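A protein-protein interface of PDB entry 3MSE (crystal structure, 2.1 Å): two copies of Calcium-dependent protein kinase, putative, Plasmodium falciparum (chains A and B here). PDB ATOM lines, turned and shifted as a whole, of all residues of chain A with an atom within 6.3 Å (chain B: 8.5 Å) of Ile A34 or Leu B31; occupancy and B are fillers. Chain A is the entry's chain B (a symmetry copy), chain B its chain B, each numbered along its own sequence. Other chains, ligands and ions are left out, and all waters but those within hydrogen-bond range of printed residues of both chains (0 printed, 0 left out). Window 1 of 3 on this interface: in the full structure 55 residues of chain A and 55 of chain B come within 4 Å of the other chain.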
ATOM      1  N   HIS A  29      -0.327 -24.462  15.232  1.00  0.00           N
ATOM      2  CA  HIS A  29       1.089 -24.131  15.239  1.00  0.00           C
ATOM      3  C   HIS A  29       1.327 -22.659  15.611  1.00  0.00           C
ATOM      4  O   HIS A  29       2.227 -22.362  16.395  1.00  0.00           O
ATOM      5  CB  HIS A  29       1.799 -24.473  13.923  1.00  0.00           C
ATOM      6  CG  HIS A  29       3.263 -24.166  13.973  1.00  0.00           C
ATOM      7  ND1 HIS A  29       3.821 -23.077  13.332  1.00  0.00           N
ATOM      8  CD2 HIS A  29       4.267 -24.746  14.675  1.00  0.00           C
ATOM      9  CE1 HIS A  29       5.115 -23.029  13.601  1.00  0.00           C
ATOM     10  NE2 HIS A  29       5.410 -24.028  14.415  1.00  0.00           N
ATOM     11  N   GLU A  30       0.501 -21.773  15.056  1.00  0.00           N
ATOM     12  CA  GLU A  30       0.552 -20.343  15.344  1.00  0.00           C
ATOM     13  C   GLU A  30       0.242 -19.991  16.811  1.00  0.00           C
ATOM     14  O   GLU A  30       0.731 -18.981  17.314  1.00  0.00           O
ATOM     15  CB  GLU A  30      -0.368 -19.571  14.389  1.00  0.00           C
ATOM     16  CG  GLU A  30       0.363 -18.655  13.404  1.00  0.00           C
ATOM     17  CD  GLU A  30       1.092 -19.399  12.296  1.00  0.00           C
ATOM     18  OE1 GLU A  30       0.454 -19.715  11.263  1.00  0.00           O
ATOM     19  OE2 GLU A  30       2.310 -19.645  12.448  1.00  0.00           O
ATOM     20  N   LEU A  31      -0.559 -20.822  17.481  1.00  0.00           N
ATOM     21  CA  LEU A  31      -0.860 -20.675  18.918  1.00  0.00           C
ATOM     22  C   LEU A  31       0.316 -21.123  19.768  1.00  0.00           C
ATOM     23  O   LEU A  31       0.611 -20.545  20.815  1.00  0.00           O
ATOM     24  CB  LEU A  31      -2.094 -21.498  19.332  1.00  0.00           C
ATOM     25  CG  LEU A  31      -3.480 -20.852  19.382  1.00  0.00           C
ATOM     26  CD1 LEU A  31      -4.442 -21.800  20.042  1.00  0.00           C
ATOM     27  CD2 LEU A  31      -3.471 -19.551  20.155  1.00  0.00           C
ATOM     28  N   SER A  32       0.967 -22.182  19.314  1.00  0.00           N
ATOM     29  CA  SER A  32       2.167 -22.673  19.939  1.00  0.00           C
ATOM     30  C   SER A  32       3.273 -21.600  19.922  1.00  0.00           C
ATOM     31  O   SER A  32       3.967 -21.402  20.916  1.00  0.00           O
ATOM     32  CB  SER A  32       2.630 -23.918  19.201  1.00  0.00           C
ATOM     33  OG  SER A  32       3.405 -24.714  20.062  1.00  0.00           O
ATOM     34  N   VAL A  33       3.420 -20.915  18.789  1.00  0.00           N
ATOM     35  CA  VAL A  33       4.463 -19.896  18.612  1.00  0.00           C
ATOM     36  C   VAL A  33       4.191 -18.756  19.580  1.00  0.00           C
ATOM     37  O   VAL A  33       5.044 -18.399  20.382  1.00  0.00           O
ATOM     38  CB  VAL A  33       4.530 -19.393  17.151  1.00  0.00           C
ATOM     39  CG1 VAL A  33       5.358 -18.087  17.039  1.00  0.00           C
ATOM     40  CG2 VAL A  33       5.100 -20.478  16.235  1.00  0.00           C
ATOM     41  N   ILE A  34       2.971 -18.229  19.520  1.00  0.00           N
ATOM     42  CA  ILE A  34       2.496 -17.203  20.432  1.00  0.00           C
ATOM     43  C   ILE A  34       2.737 -17.587  21.889  1.00  0.00           C
ATOM     44  O   ILE A  34       3.297 -16.800  22.660  1.00  0.00           O
ATOM     45  CB  ILE A  34       1.005 -16.898  20.156  1.00  0.00           C
ATOM     46  CG1 ILE A  34       0.882 -16.173  18.810  1.00  0.00           C
ATOM     47  CG2 ILE A  34       0.387 -16.093  21.296  1.00  0.00           C
ATOM     48  CD1 ILE A  34      -0.525 -16.059  18.252  1.00  0.00           C
ATOM     49  N   ASN A  35       2.340 -18.804  22.248  1.00  0.00           N
ATOM     50  CA  ASN A  35       2.460 -19.325  23.606  1.00  0.00           C
ATOM     51  C   ASN A  35       3.911 -19.476  24.074  1.00  0.00           C
ATOM     52  O   ASN A  35       4.191 -19.402  25.270  1.00  0.00           O
ATOM     53  CB  ASN A  35       1.721 -20.673  23.712  1.00  0.00           C
ATOM     54  CG  ASN A  35       1.998 -21.406  25.018  1.00  0.00           C
ATOM     55  OD1 ASN A  35       2.740 -22.391  25.054  1.00  0.00           O
ATOM     56  ND2 ASN A  35       1.415 -20.920  26.094  1.00  0.00           N
ATOM     57  N   ASN A  36       4.825 -19.720  23.137  1.00  0.00           N
ATOM     58  CA  ASN A  36       6.252 -19.768  23.472  1.00  0.00           C
ATOM     59  C   ASN A  36       6.766 -18.394  23.882  1.00  0.00           C
ATOM     60  O   ASN A  36       7.465 -18.280  24.890  1.00  0.00           O
ATOM     61  CB  ASN A  36       7.087 -20.333  22.318  1.00  0.00           C
ATOM     62  CG  ASN A  36       6.872 -21.821  22.116  1.00  0.00           C
ATOM     63  OD1 ASN A  36       6.774 -22.591  23.079  1.00  0.00           O
ATOM     64  ND2 ASN A  36       6.806 -22.238  20.855  1.00  0.00           N
ATOM     65  N   HIS A  37       6.405 -17.365  23.108  1.00  0.00           N
ATOM     66  CA  HIS A  37       6.716 -15.965  23.451  1.00  0.00           C
ATOM     67  C   HIS A  37       6.177 -15.628  24.840  1.00  0.00           C
ATOM     68  O   HIS A  37       6.912 -15.113  25.686  1.00  0.00           O
ATOM     69  CB  HIS A  37       6.146 -14.976  22.418  1.00  0.00           C
ATOM     70  CG  HIS A  37       6.788 -15.050  21.065  1.00  0.00           C
ATOM     71  ND1 HIS A  37       8.155 -15.039  20.877  1.00  0.00           N
ATOM     72  CD2 HIS A  37       6.242 -15.091  19.824  1.00  0.00           C
ATOM     73  CE1 HIS A  37       8.423 -15.108  19.585  1.00  0.00           C
ATOM     74  NE2 HIS A  37       7.280 -15.135  18.923  1.00  0.00           N
ATOM     75  N   ILE A  38       4.905 -15.951  25.087  1.00  0.00           N
ATOM     76  CA  ILE A  38       4.292 -15.692  26.386  1.00  0.00           C
ATOM     77  C   ILE A  38       4.996 -16.441  27.518  1.00  0.00           C
ATOM     78  O   ILE A  38       5.146 -15.909  28.624  1.00  0.00           O
ATOM     79  CB  ILE A  38       2.781 -16.003  26.391  1.00  0.00           C
ATOM     80  CG1 ILE A  38       2.057 -15.086  25.409  1.00  0.00           C
ATOM     81  CG2 ILE A  38       2.196 -15.844  27.795  1.00  0.00           C
ATOM     82  CD1 ILE A  38       0.602 -15.432  25.226  1.00  0.00           C
ATOM     83  N   LYS A  39       5.434 -17.666  27.246  1.00  0.00           N
ATOM     84  CA  LYS A  39       6.170 -18.449  28.231  1.00  0.00           C
ATOM     85  C   LYS A  39       7.473 -17.735  28.637  1.00  0.00           C
ATOM     86  O   LYS A  39       7.791 -17.650  29.826  1.00  0.00           O
ATOM     87  CB  LYS A  39       6.464 -19.852  27.692  1.00  0.00           C
ATOM     88  CG  LYS A  39       6.838 -20.883  28.752  1.00  0.00           C
ATOM     89  CD  LYS A  39       6.858 -22.323  28.184  1.00  0.00           C
ATOM     90  CE  LYS A  39       5.475 -22.763  27.667  1.00  0.00           C
ATOM     91  NZ  LYS A  39       4.448 -22.947  28.751  1.00  0.00           N
ATOM     92  N   MET A  96       3.351  -7.691  30.432  1.00  0.00           N
ATOM     93  CA  MET A  96       3.318  -8.447  29.224  1.00  0.00           C
ATOM     94  C   MET A  96       2.868  -7.609  28.009  1.00  0.00           C
ATOM     95  O   MET A  96       3.341  -7.824  26.877  1.00  0.00           O
ATOM     96  CB  MET A  96       2.495  -9.711  29.486  1.00  0.00           C
ATOM     97  CG  MET A  96       1.290  -9.840  28.696  1.00  0.00           C
ATOM     98  SD  MET A  96       1.877 -10.931  27.447  1.00  0.00           S
ATOM     99  CE  MET A  96       0.737 -10.426  26.173  1.00  0.00           C
ATOM    100  N   TYR A 100       5.460  -7.775  24.682  1.00  0.00           N
ATOM    101  CA  TYR A 100       5.021  -8.602  23.557  1.00  0.00           C
ATOM    102  C   TYR A 100       5.117  -7.852  22.243  1.00  0.00           C
ATOM    103  O   TYR A 100       4.741  -6.688  22.169  1.00  0.00           O
ATOM    104  CB  TYR A 100       3.578  -9.095  23.785  1.00  0.00           C
ATOM    105  CG  TYR A 100       3.095 -10.101  22.767  1.00  0.00           C
ATOM    106  CD1 TYR A 100       3.439 -11.454  22.865  1.00  0.00           C
ATOM    107  CD2 TYR A 100       2.286  -9.703  21.707  1.00  0.00           C
ATOM    108  CE1 TYR A 100       2.987 -12.388  21.903  1.00  0.00           C
ATOM    109  CE2 TYR A 100       1.831 -10.620  20.754  1.00  0.00           C
ATOM    110  CZ  TYR A 100       2.182 -11.947  20.859  1.00  0.00           C
ATOM    111  OH  TYR A 100       1.728 -12.832  19.910  1.00  0.00           O
ATOM    112  N   TRP A 102       3.643  -6.851  19.102  1.00  0.00           N
ATOM    113  CA  TRP A 102       2.282  -6.789  18.576  1.00  0.00           C
ATOM    114  C   TRP A 102       2.209  -6.788  17.046  1.00  0.00           C
ATOM    115  O   TRP A 102       1.157  -7.068  16.477  1.00  0.00           O
ATOM    116  CB  TRP A 102       1.523  -5.608  19.209  1.00  0.00           C
ATOM    117  CG  TRP A 102       1.287  -5.863  20.680  1.00  0.00           C
ATOM    118  CD1 TRP A 102       2.003  -5.363  21.727  1.00  0.00           C
ATOM    119  CD2 TRP A 102       0.319  -6.751  21.242  1.00  0.00           C
ATOM    120  NE1 TRP A 102       1.529  -5.869  22.918  1.00  0.00           N
ATOM    121  CE2 TRP A 102       0.491  -6.724  22.644  1.00  0.00           C
ATOM    122  CE3 TRP A 102      -0.686  -7.562  20.699  1.00  0.00           C
ATOM    123  CZ2 TRP A 102      -0.315  -7.477  23.510  1.00  0.00           C
ATOM    124  CZ3 TRP A 102      -1.483  -8.308  21.560  1.00  0.00           C
ATOM    125  CH2 TRP A 102      -1.299  -8.251  22.947  1.00  0.00           C
ATOM    126  N   ILE A 105      -0.289  -8.861  14.423  1.00  0.00           N
ATOM    127  CA  ILE A 105      -1.259  -9.527  15.308  1.00  0.00           C
ATOM    128  C   ILE A 105      -2.626  -9.662  14.631  1.00  0.00           C
ATOM    129  O   ILE A 105      -3.052  -8.758  13.912  1.00  0.00           O
ATOM    130  CB  ILE A 105      -1.405  -8.784  16.699  1.00  0.00           C
ATOM    131  CG1 ILE A 105      -2.044  -9.687  17.768  1.00  0.00           C
ATOM    132  CG2 ILE A 105      -2.172  -7.448  16.570  1.00  0.00           C
ATOM    133  CD1 ILE A 105      -1.092 -10.688  18.408  1.00  0.00           C
ATOM    134  N   PHE A 109      -5.643 -15.286  12.790  1.00  0.00           N
ATOM    135  CA  PHE A 109      -5.294 -16.713  12.668  1.00  0.00           C
ATOM    136  C   PHE A 109      -5.706 -17.329  11.344  1.00  0.00           C
ATOM    137  O   PHE A 109      -4.961 -18.119  10.762  1.00  0.00           O
ATOM    138  CB  PHE A 109      -5.941 -17.513  13.787  1.00  0.00           C
ATOM    139  CG  PHE A 109      -5.294 -17.320  15.113  1.00  0.00           C
ATOM    140  CD1 PHE A 109      -5.733 -16.312  15.971  1.00  0.00           C
ATOM    141  CD2 PHE A 109      -4.247 -18.145  15.510  1.00  0.00           C
ATOM    142  CE1 PHE A 109      -5.139 -16.133  17.220  1.00  0.00           C
ATOM    143  CE2 PHE A 109      -3.646 -17.977  16.743  1.00  0.00           C
ATOM    144  CZ  PHE A 109      -4.093 -16.967  17.607  1.00  0.00           C
ATOM    145  N   ILE B  24      -3.683  -1.571  24.076  1.00  0.00           N
ATOM    146  CA  ILE B  24      -2.798  -2.742  24.051  1.00  0.00           C
ATOM    147  C   ILE B  24      -3.072  -3.667  25.250  1.00  0.00           C
ATOM    148  O   ILE B  24      -3.060  -4.886  25.096  1.00  0.00           O
ATOM    149  CB  ILE B  24      -1.254  -2.358  24.039  1.00  0.00           C
ATOM    150  CG1 ILE B  24      -0.842  -1.597  22.763  1.00  0.00           C
ATOM    151  CG2 ILE B  24      -0.411  -3.592  24.237  1.00  0.00           C
ATOM    152  CD1 ILE B  24      -0.716  -2.464  21.493  1.00  0.00           C
ATOM    153  N   ASN B  25      -3.290  -3.097  26.437  1.00  0.00           N
ATOM    154  CA  ASN B  25      -3.607  -3.919  27.637  1.00  0.00           C
ATOM    155  C   ASN B  25      -4.891  -4.777  27.531  1.00  0.00           C
ATOM    156  O   ASN B  25      -4.934  -5.894  28.052  1.00  0.00           O
ATOM    157  CB  ASN B  25      -3.654  -3.068  28.912  1.00  0.00           C
ATOM    158  CG  ASN B  25      -2.302  -2.968  29.590  1.00  0.00           C
ATOM    159  OD1 ASN B  25      -2.033  -3.681  30.553  1.00  0.00           O
ATOM    160  ND2 ASN B  25      -1.436  -2.082  29.080  1.00  0.00           N
ATOM    161  N   ILE B  26      -5.895  -4.253  26.833  1.00  0.00           N
ATOM    162  CA  ILE B  26      -7.115  -5.013  26.512  1.00  0.00           C
ATOM    163  C   ILE B  26      -6.770  -6.268  25.713  1.00  0.00           C
ATOM    164  O   ILE B  26      -7.184  -7.384  26.061  1.00  0.00           O
ATOM    165  CB  ILE B  26      -8.155  -4.157  25.726  1.00  0.00           C
ATOM    166  CG1 ILE B  26      -8.673  -3.021  26.597  1.00  0.00           C
ATOM    167  CG2 ILE B  26      -9.334  -5.042  25.215  1.00  0.00           C
ATOM    168  CD1 ILE B  26      -9.276  -1.866  25.784  1.00  0.00           C
ATOM    169  N   MET B  27      -5.982  -6.087  24.657  1.00  0.00           N
ATOM    170  CA  MET B  27      -5.497  -7.218  23.869  1.00  0.00           C
ATOM    171  C   MET B  27      -4.606  -8.150  24.680  1.00  0.00           C
ATOM    172  O   MET B  27      -4.650  -9.377  24.509  1.00  0.00           O
ATOM    173  CB  MET B  27      -4.767  -6.713  22.632  1.00  0.00           C
ATOM    174  CG  MET B  27      -5.686  -6.077  21.618  1.00  0.00           C
ATOM    175  SD  MET B  27      -4.803  -5.750  20.078  1.00  0.00           S
ATOM    176  CE  MET B  27      -3.947  -4.253  20.526  1.00  0.00           C
ATOM    177  N   ALA B  28      -3.805  -7.571  25.573  1.00  0.00           N
ATOM    178  CA  ALA B  28      -2.915  -8.353  26.424  1.00  0.00           C
ATOM    179  C   ALA B  28      -3.703  -9.261  27.356  1.00  0.00           C
ATOM    180  O   ALA B  28      -3.283 -10.389  27.642  1.00  0.00           O
ATOM    181  CB  ALA B  28      -2.008  -7.452  27.226  1.00  0.00           C
ATOM    182  N   HIS B  29      -4.830  -8.755  27.851  1.00  0.00           N
ATOM    183  CA  HIS B  29      -5.709  -9.586  28.658  1.00  0.00           C
ATOM    184  C   HIS B  29      -6.221 -10.804  27.871  1.00  0.00           C
ATOM    185  O   HIS B  29      -6.250 -11.912  28.406  1.00  0.00           O
ATOM    186  CB  HIS B  29      -6.883  -8.813  29.270  1.00  0.00           C
ATOM    187  CG  HIS B  29      -7.746  -9.680  30.132  1.00  0.00           C
ATOM    188  ND1 HIS B  29      -8.989 -10.130  29.734  1.00  0.00           N
ATOM    189  CD2 HIS B  29      -7.498 -10.266  31.329  1.00  0.00           C
ATOM    190  CE1 HIS B  29      -9.488 -10.919  30.671  1.00  0.00           C
ATOM    191  NE2 HIS B  29      -8.601 -11.020  31.648  1.00  0.00           N
ATOM    192  N   GLU B  30      -6.591 -10.576  26.613  1.00  0.00           N
ATOM    193  CA  GLU B  30      -7.047 -11.629  25.710  1.00  0.00           C
ATOM    194  C   GLU B  30      -5.976 -12.689  25.397  1.00  0.00           C
ATOM    195  O   GLU B  30      -6.316 -13.839  25.120  1.00  0.00           O
ATOM    196  CB  GLU B  30      -7.610 -11.020  24.418  1.00  0.00           C
ATOM    197  CG  GLU B  30      -9.116 -11.214  24.227  1.00  0.00           C
ATOM    198  CD  GLU B  30      -9.968 -10.354  25.147  1.00  0.00           C
ATOM    199  OE1 GLU B  30     -10.247  -9.184  24.790  1.00  0.00           O
ATOM    200  OE2 GLU B  30     -10.381 -10.858  26.216  1.00  0.00           O
ATOM    201  N   LEU B  31      -4.700 -12.301  25.447  1.00  0.00           N
ATOM    202  CA  LEU B  31      -3.564 -13.226  25.277  1.00  0.00           C
ATOM    203  C   LEU B  31      -3.356 -14.066  26.526  1.00  0.00           C
ATOM    204  O   LEU B  31      -3.005 -15.246  26.456  1.00  0.00           O
ATOM    205  CB  LEU B  31      -2.253 -12.475  24.980  1.00  0.00           C
ATOM    206  CG  LEU B  31      -1.784 -12.266  23.538  1.00  0.00           C
ATOM    207  CD1 LEU B  31      -0.380 -11.730  23.550  1.00  0.00           C
ATOM    208  CD2 LEU B  31      -1.808 -13.553  22.743  1.00  0.00           C
ATOM    209  N   SER B  32      -3.552 -13.431  27.670  1.00  0.00           N
ATOM    210  CA  SER B  32      -3.501 -14.106  28.940  1.00  0.00           C
ATOM    211  C   SER B  32      -4.568 -15.215  29.016  1.00  0.00           C
ATOM    212  O   SER B  32      -4.294 -16.315  29.490  1.00  0.00           O
ATOM    213  CB  SER B  32      -3.723 -13.086  30.045  1.00  0.00           C
ATOM    214  OG  SER B  32      -3.142 -13.552  31.238  1.00  0.00           O
ATOM    215  N   VAL B  33      -5.775 -14.912  28.542  1.00  0.00           N
ATOM    216  CA  VAL B  33      -6.902 -15.854  28.592  1.00  0.00           C
ATOM    217  C   VAL B  33      -6.566 -17.052  27.721  1.00  0.00           C
ATOM    218  O   VAL B  33      -6.585 -18.186  28.183  1.00  0.00           O
ATOM    219  CB  VAL B  33      -8.225 -15.186  28.148  1.00  0.00           C
ATOM    220  CG1 VAL B  33      -9.322 -16.243  27.853  1.00  0.00           C
ATOM    221  CG2 VAL B  33      -8.703 -14.187  29.204  1.00  0.00           C
ATOM    222  N   ILE B  34      -6.211 -16.774  26.469  1.00  0.00           N
ATOM    223  CA  ILE B  34      -5.758 -17.779  25.523  1.00  0.00           C
ATOM    224  C   ILE B  34      -4.652 -18.651  26.109  1.00  0.00           C
ATOM    225  O   ILE B  34      -4.733 -19.883  26.063  1.00  0.00           O
ATOM    226  CB  ILE B  34      -5.321 -17.103  24.202  1.00  0.00           C
ATOM    227  CG1 ILE B  34      -6.561 -16.559  23.482  1.00  0.00           C
ATOM    228  CG2 ILE B  34      -4.530 -18.069  23.324  1.00  0.00           C
ATOM    229  CD1 ILE B  34      -6.286 -15.618  22.323  1.00  0.00           C
ATOM    230  N   ASN B  35      -3.641 -18.005  26.683  1.00  0.00           N
ATOM    231  CA  ASN B  35      -2.482 -18.676  27.263  1.00  0.00           C
ATOM    232  C   ASN B  35      -2.827 -19.554  28.470  1.00  0.00           C
ATOM    233  O   ASN B  35      -2.136 -20.534  28.748  1.00  0.00           O
ATOM    234  CB  ASN B  35      -1.418 -17.631  27.650  1.00  0.00           C
ATOM    235  CG  ASN B  35      -0.283 -18.213  28.484  1.00  0.00           C
ATOM    236  OD1 ASN B  35      -0.202 -17.994  29.695  1.00  0.00           O
ATOM    237  ND2 ASN B  35       0.586 -18.964  27.842  1.00  0.00           N
ATOM    238  N   ASN B  36      -3.875 -19.185  29.204  1.00  0.00           N
ATOM    239  CA  ASN B  36      -4.352 -20.022  30.310  1.00  0.00           C
ATOM    240  C   ASN B  36      -4.936 -21.333  29.795  1.00  0.00           C
ATOM    241  O   ASN B  36      -4.617 -22.394  30.330  1.00  0.00           O
ATOM    242  CB  ASN B  36      -5.374 -19.284  31.181  1.00  0.00           C
ATOM    243  CG  ASN B  36      -4.744 -18.183  32.012  1.00  0.00           C
ATOM    244  OD1 ASN B  36      -3.648 -18.342  32.562  1.00  0.00           O
ATOM    245  ND2 ASN B  36      -5.441 -17.055  32.117  1.00  0.00           N
ATOM    246  N   HIS B  37      -5.771 -21.246  28.755  1.00  0.00           N
ATOM    247  CA  HIS B  37      -6.310 -22.435  28.068  1.00  0.00           C
ATOM    248  C   HIS B  37      -5.169 -23.333  27.591  1.00  0.00           C
ATOM    249  O   HIS B  37      -5.165 -24.535  27.864  1.00  0.00           O
ATOM    250  CB  HIS B  37      -7.207 -22.057  26.875  1.00  0.00           C
ATOM    251  CG  HIS B  37      -8.492 -21.384  27.252  1.00  0.00           C
ATOM    252  ND1 HIS B  37      -9.345 -21.873  28.220  1.00  0.00           N
ATOM    253  CD2 HIS B  37      -9.094 -20.275  26.754  1.00  0.00           C
ATOM    254  CE1 HIS B  37     -10.394 -21.077  28.329  1.00  0.00           C
ATOM    255  NE2 HIS B  37     -10.269 -20.102  27.447  1.00  0.00           N
ATOM    256  N   ILE B  38      -4.184 -22.741  26.909  1.00  0.00           N
ATOM    257  CA  ILE B  38      -3.034 -23.500  26.422  1.00  0.00           C
ATOM    258  C   ILE B  38      -2.242 -24.145  27.559  1.00  0.00           C
ATOM    259  O   ILE B  38      -1.753 -25.273  27.422  1.00  0.00           O
ATOM    260  CB  ILE B  38      -2.107 -22.647  25.533  1.00  0.00           C
ATOM    261  CG1 ILE B  38      -2.855 -22.192  24.282  1.00  0.00           C
ATOM    262  CG2 ILE B  38      -0.851 -23.430  25.145  1.00  0.00           C
ATOM    263  CD1 ILE B  38      -2.077 -21.216  23.439  1.00  0.00           C
ATOM    264  N   TYR B 100      -8.422 -27.488  21.729  1.00  0.00           N
ATOM    265  CA  TYR B 100      -8.643 -26.045  21.853  1.00  0.00           C
ATOM    266  C   TYR B 100      -9.984 -25.636  21.278  1.00  0.00           C
ATOM    267  O   TYR B 100     -10.364 -26.096  20.207  1.00  0.00           O
ATOM    268  CB  TYR B 100      -7.507 -25.267  21.161  1.00  0.00           C
ATOM    269  CG  TYR B 100      -7.547 -23.774  21.385  1.00  0.00           C
ATOM    270  CD1 TYR B 100      -7.049 -23.205  22.564  1.00  0.00           C
ATOM    271  CD2 TYR B 100      -8.075 -22.926  20.418  1.00  0.00           C
ATOM    272  CE1 TYR B 100      -7.097 -21.806  22.769  1.00  0.00           C
ATOM    273  CE2 TYR B 100      -8.122 -21.541  20.610  1.00  0.00           C
ATOM    274  CZ  TYR B 100      -7.635 -20.996  21.775  1.00  0.00           C
ATOM    275  OH  TYR B 100      -7.694 -19.632  21.947  1.00  0.00           O
ATOM    276  N   ILE B 105     -12.414 -17.328  17.219  1.00  0.00           N
ATOM    277  CA  ILE B 105     -10.968 -17.105  17.055  1.00  0.00           C
ATOM    278  C   ILE B 105     -10.689 -15.956  16.082  1.00  0.00           C
ATOM    279  O   ILE B 105     -11.395 -15.806  15.085  1.00  0.00           O
ATOM    280  CB  ILE B 105     -10.211 -18.417  16.590  1.00  0.00           C
ATOM    281  CG1 ILE B 105      -8.697 -18.329  16.847  1.00  0.00           C
ATOM    282  CG2 ILE B 105     -10.504 -18.766  15.112  1.00  0.00           C
ATOM    283  CD1 ILE B 105      -8.280 -18.604  18.285  1.00  0.00           C
ATOM    284  N   PHE B 109      -7.946 -10.078  17.509  1.00  0.00           N
ATOM    285  CA  PHE B 109      -7.578  -9.318  18.717  1.00  0.00           C
ATOM    286  C   PHE B 109      -8.052  -7.877  18.698  1.00  0.00           C
ATOM    287  O   PHE B 109      -8.510  -7.355  19.715  1.00  0.00           O
ATOM    288  CB  PHE B 109      -6.070  -9.320  18.905  1.00  0.00           C
ATOM    289  CG  PHE B 109      -5.527 -10.622  19.381  1.00  0.00           C
ATOM    290  CD1 PHE B 109      -5.125 -11.595  18.468  1.00  0.00           C
ATOM    291  CD2 PHE B 109      -5.413 -10.878  20.744  1.00  0.00           C
ATOM    292  CE1 PHE B 109      -4.606 -12.812  18.907  1.00  0.00           C
ATOM    293  CE2 PHE B 109      -4.903 -12.081  21.195  1.00  0.00           C
ATOM    294  CZ  PHE B 109      -4.494 -13.056  20.275  1.00  0.00           C
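Among the printed residues, merely in contact across the chains: Leu A31 with Ile B34 (3.7 Å), Leu A31 with Ile B38 (3.8 Å), Leu A31 with Tyr B100 (3.7 Å), Ile A34 with Leu B31 (3.7 Å), Asn A35 with Ile B38 (3.5 Å), Ile A38 with Leu B31 (3.8 Å), Ile A38 with Asn B35 (3.5 Å), Met A96 with Leu B31 (3.1 Å), Tyr A100 with Leu B31 (3.7 Å), Trp A102 with Ile B24 (3.3 Å), Trp A102 with Met B27 (3.7 Å), Trp A102 with Ala B28 (3.7 Å), Trp A102 with Leu B31 (3.6 Å), Ile A105 with Phe B109 (3.7 Å), Phe A109 with Ile B105 (3.7 Å) and Phe A109 with Phe B109 (3.8 Å).
Of the 18 printed residues of chain B, 10 touch a printed residue of chain A. Hydrophobic or aromatic side chains of chain B that line the printed part of chain A: Ile B24, Met B27, Leu B31, Ile B34, Ile B38, Tyr B100, Ile B105 and Phe B109. Of the 16 printed residues of chain A, 9 touch a printed residue of chain B. Printed residues of chain A that touch a printed residue of chain B: Leu A31, Ile A34, Asn A35, Ile A38, Met A96, Tyr A100, Trp A102, Ile A105 and Phe A109. Hydrophobic or aromatic side chains of chain A within 4 Å of the printed part of chain B: Leu A31, Ile A34, Ile A38, Met A96, Tyr A100, Trp A102, Ile A105 and Phe A109. Along chain A the printed residues that touch a printed residue of chain B span positions 31 to 109. Among the printed residues, 17 pairs touch across the chains. Among the printed residues, no Asp or Glu carboxylate lies within 4 Å of a Lys or Arg side-chain nitrogen of the other chain.
ND2 of Asn B35 lies close to ND2 of Asn A35 (2.8 Å).
Ile A34 touches just one residue of chain B: Leu B31 (3.7 Å). Printed residues of chain B within 4 Å of Asn A35: Asn B35 (2.8 Å) and Ile B38 (3.5 Å). Printed residues of chain B within 4 Å of Ile A38: Leu B31 and Asn B35. Printed residues of chain B within 4 Å of Met A96: Leu B31 (3.1 Å). Of chain A, only Ile A34, Ile A38, Met A96, Tyr A100 and Trp A102 come within 4 Å of Leu B31. Ser B32 touches none of the printed residues of chain A. Of the printed residues of chain A, Ile B38 touches Leu A31 and Asn A35. Of the printed residues of chain A, Ile B105 touches Phe A109. The nearest residue of chain B that does not touch Ile A34 is Phe B109 (5.3 Å). The nearest residue of chain A that does not touch Leu B31 is Ile A105 (5.2 Å). The nearest printed residue of chain B that does not touch Trp A102 is Phe B109 (4.8 Å).
NE1 of Trp A102 lies close to O of Tyr A100, 3.4 Å away.
Leu A31 touches Ile B38, and with the chains exchanged Ile A38 touches Leu B31. Leu A31 touches Tyr B100, and with the chains exchanged Tyr A100 touches Leu B31. Asn A35 touches Ile B38, and with the chains exchanged Ile A38 touches Asn B35. Ile A105 touches Phe B109, and with the chains exchanged Phe A109 touches Ile B105. 13 positions are printed for both chains. Of the 17 pairs that touch across the chains among the printed residues, 12 have their exchanged pair printed and touching as well.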
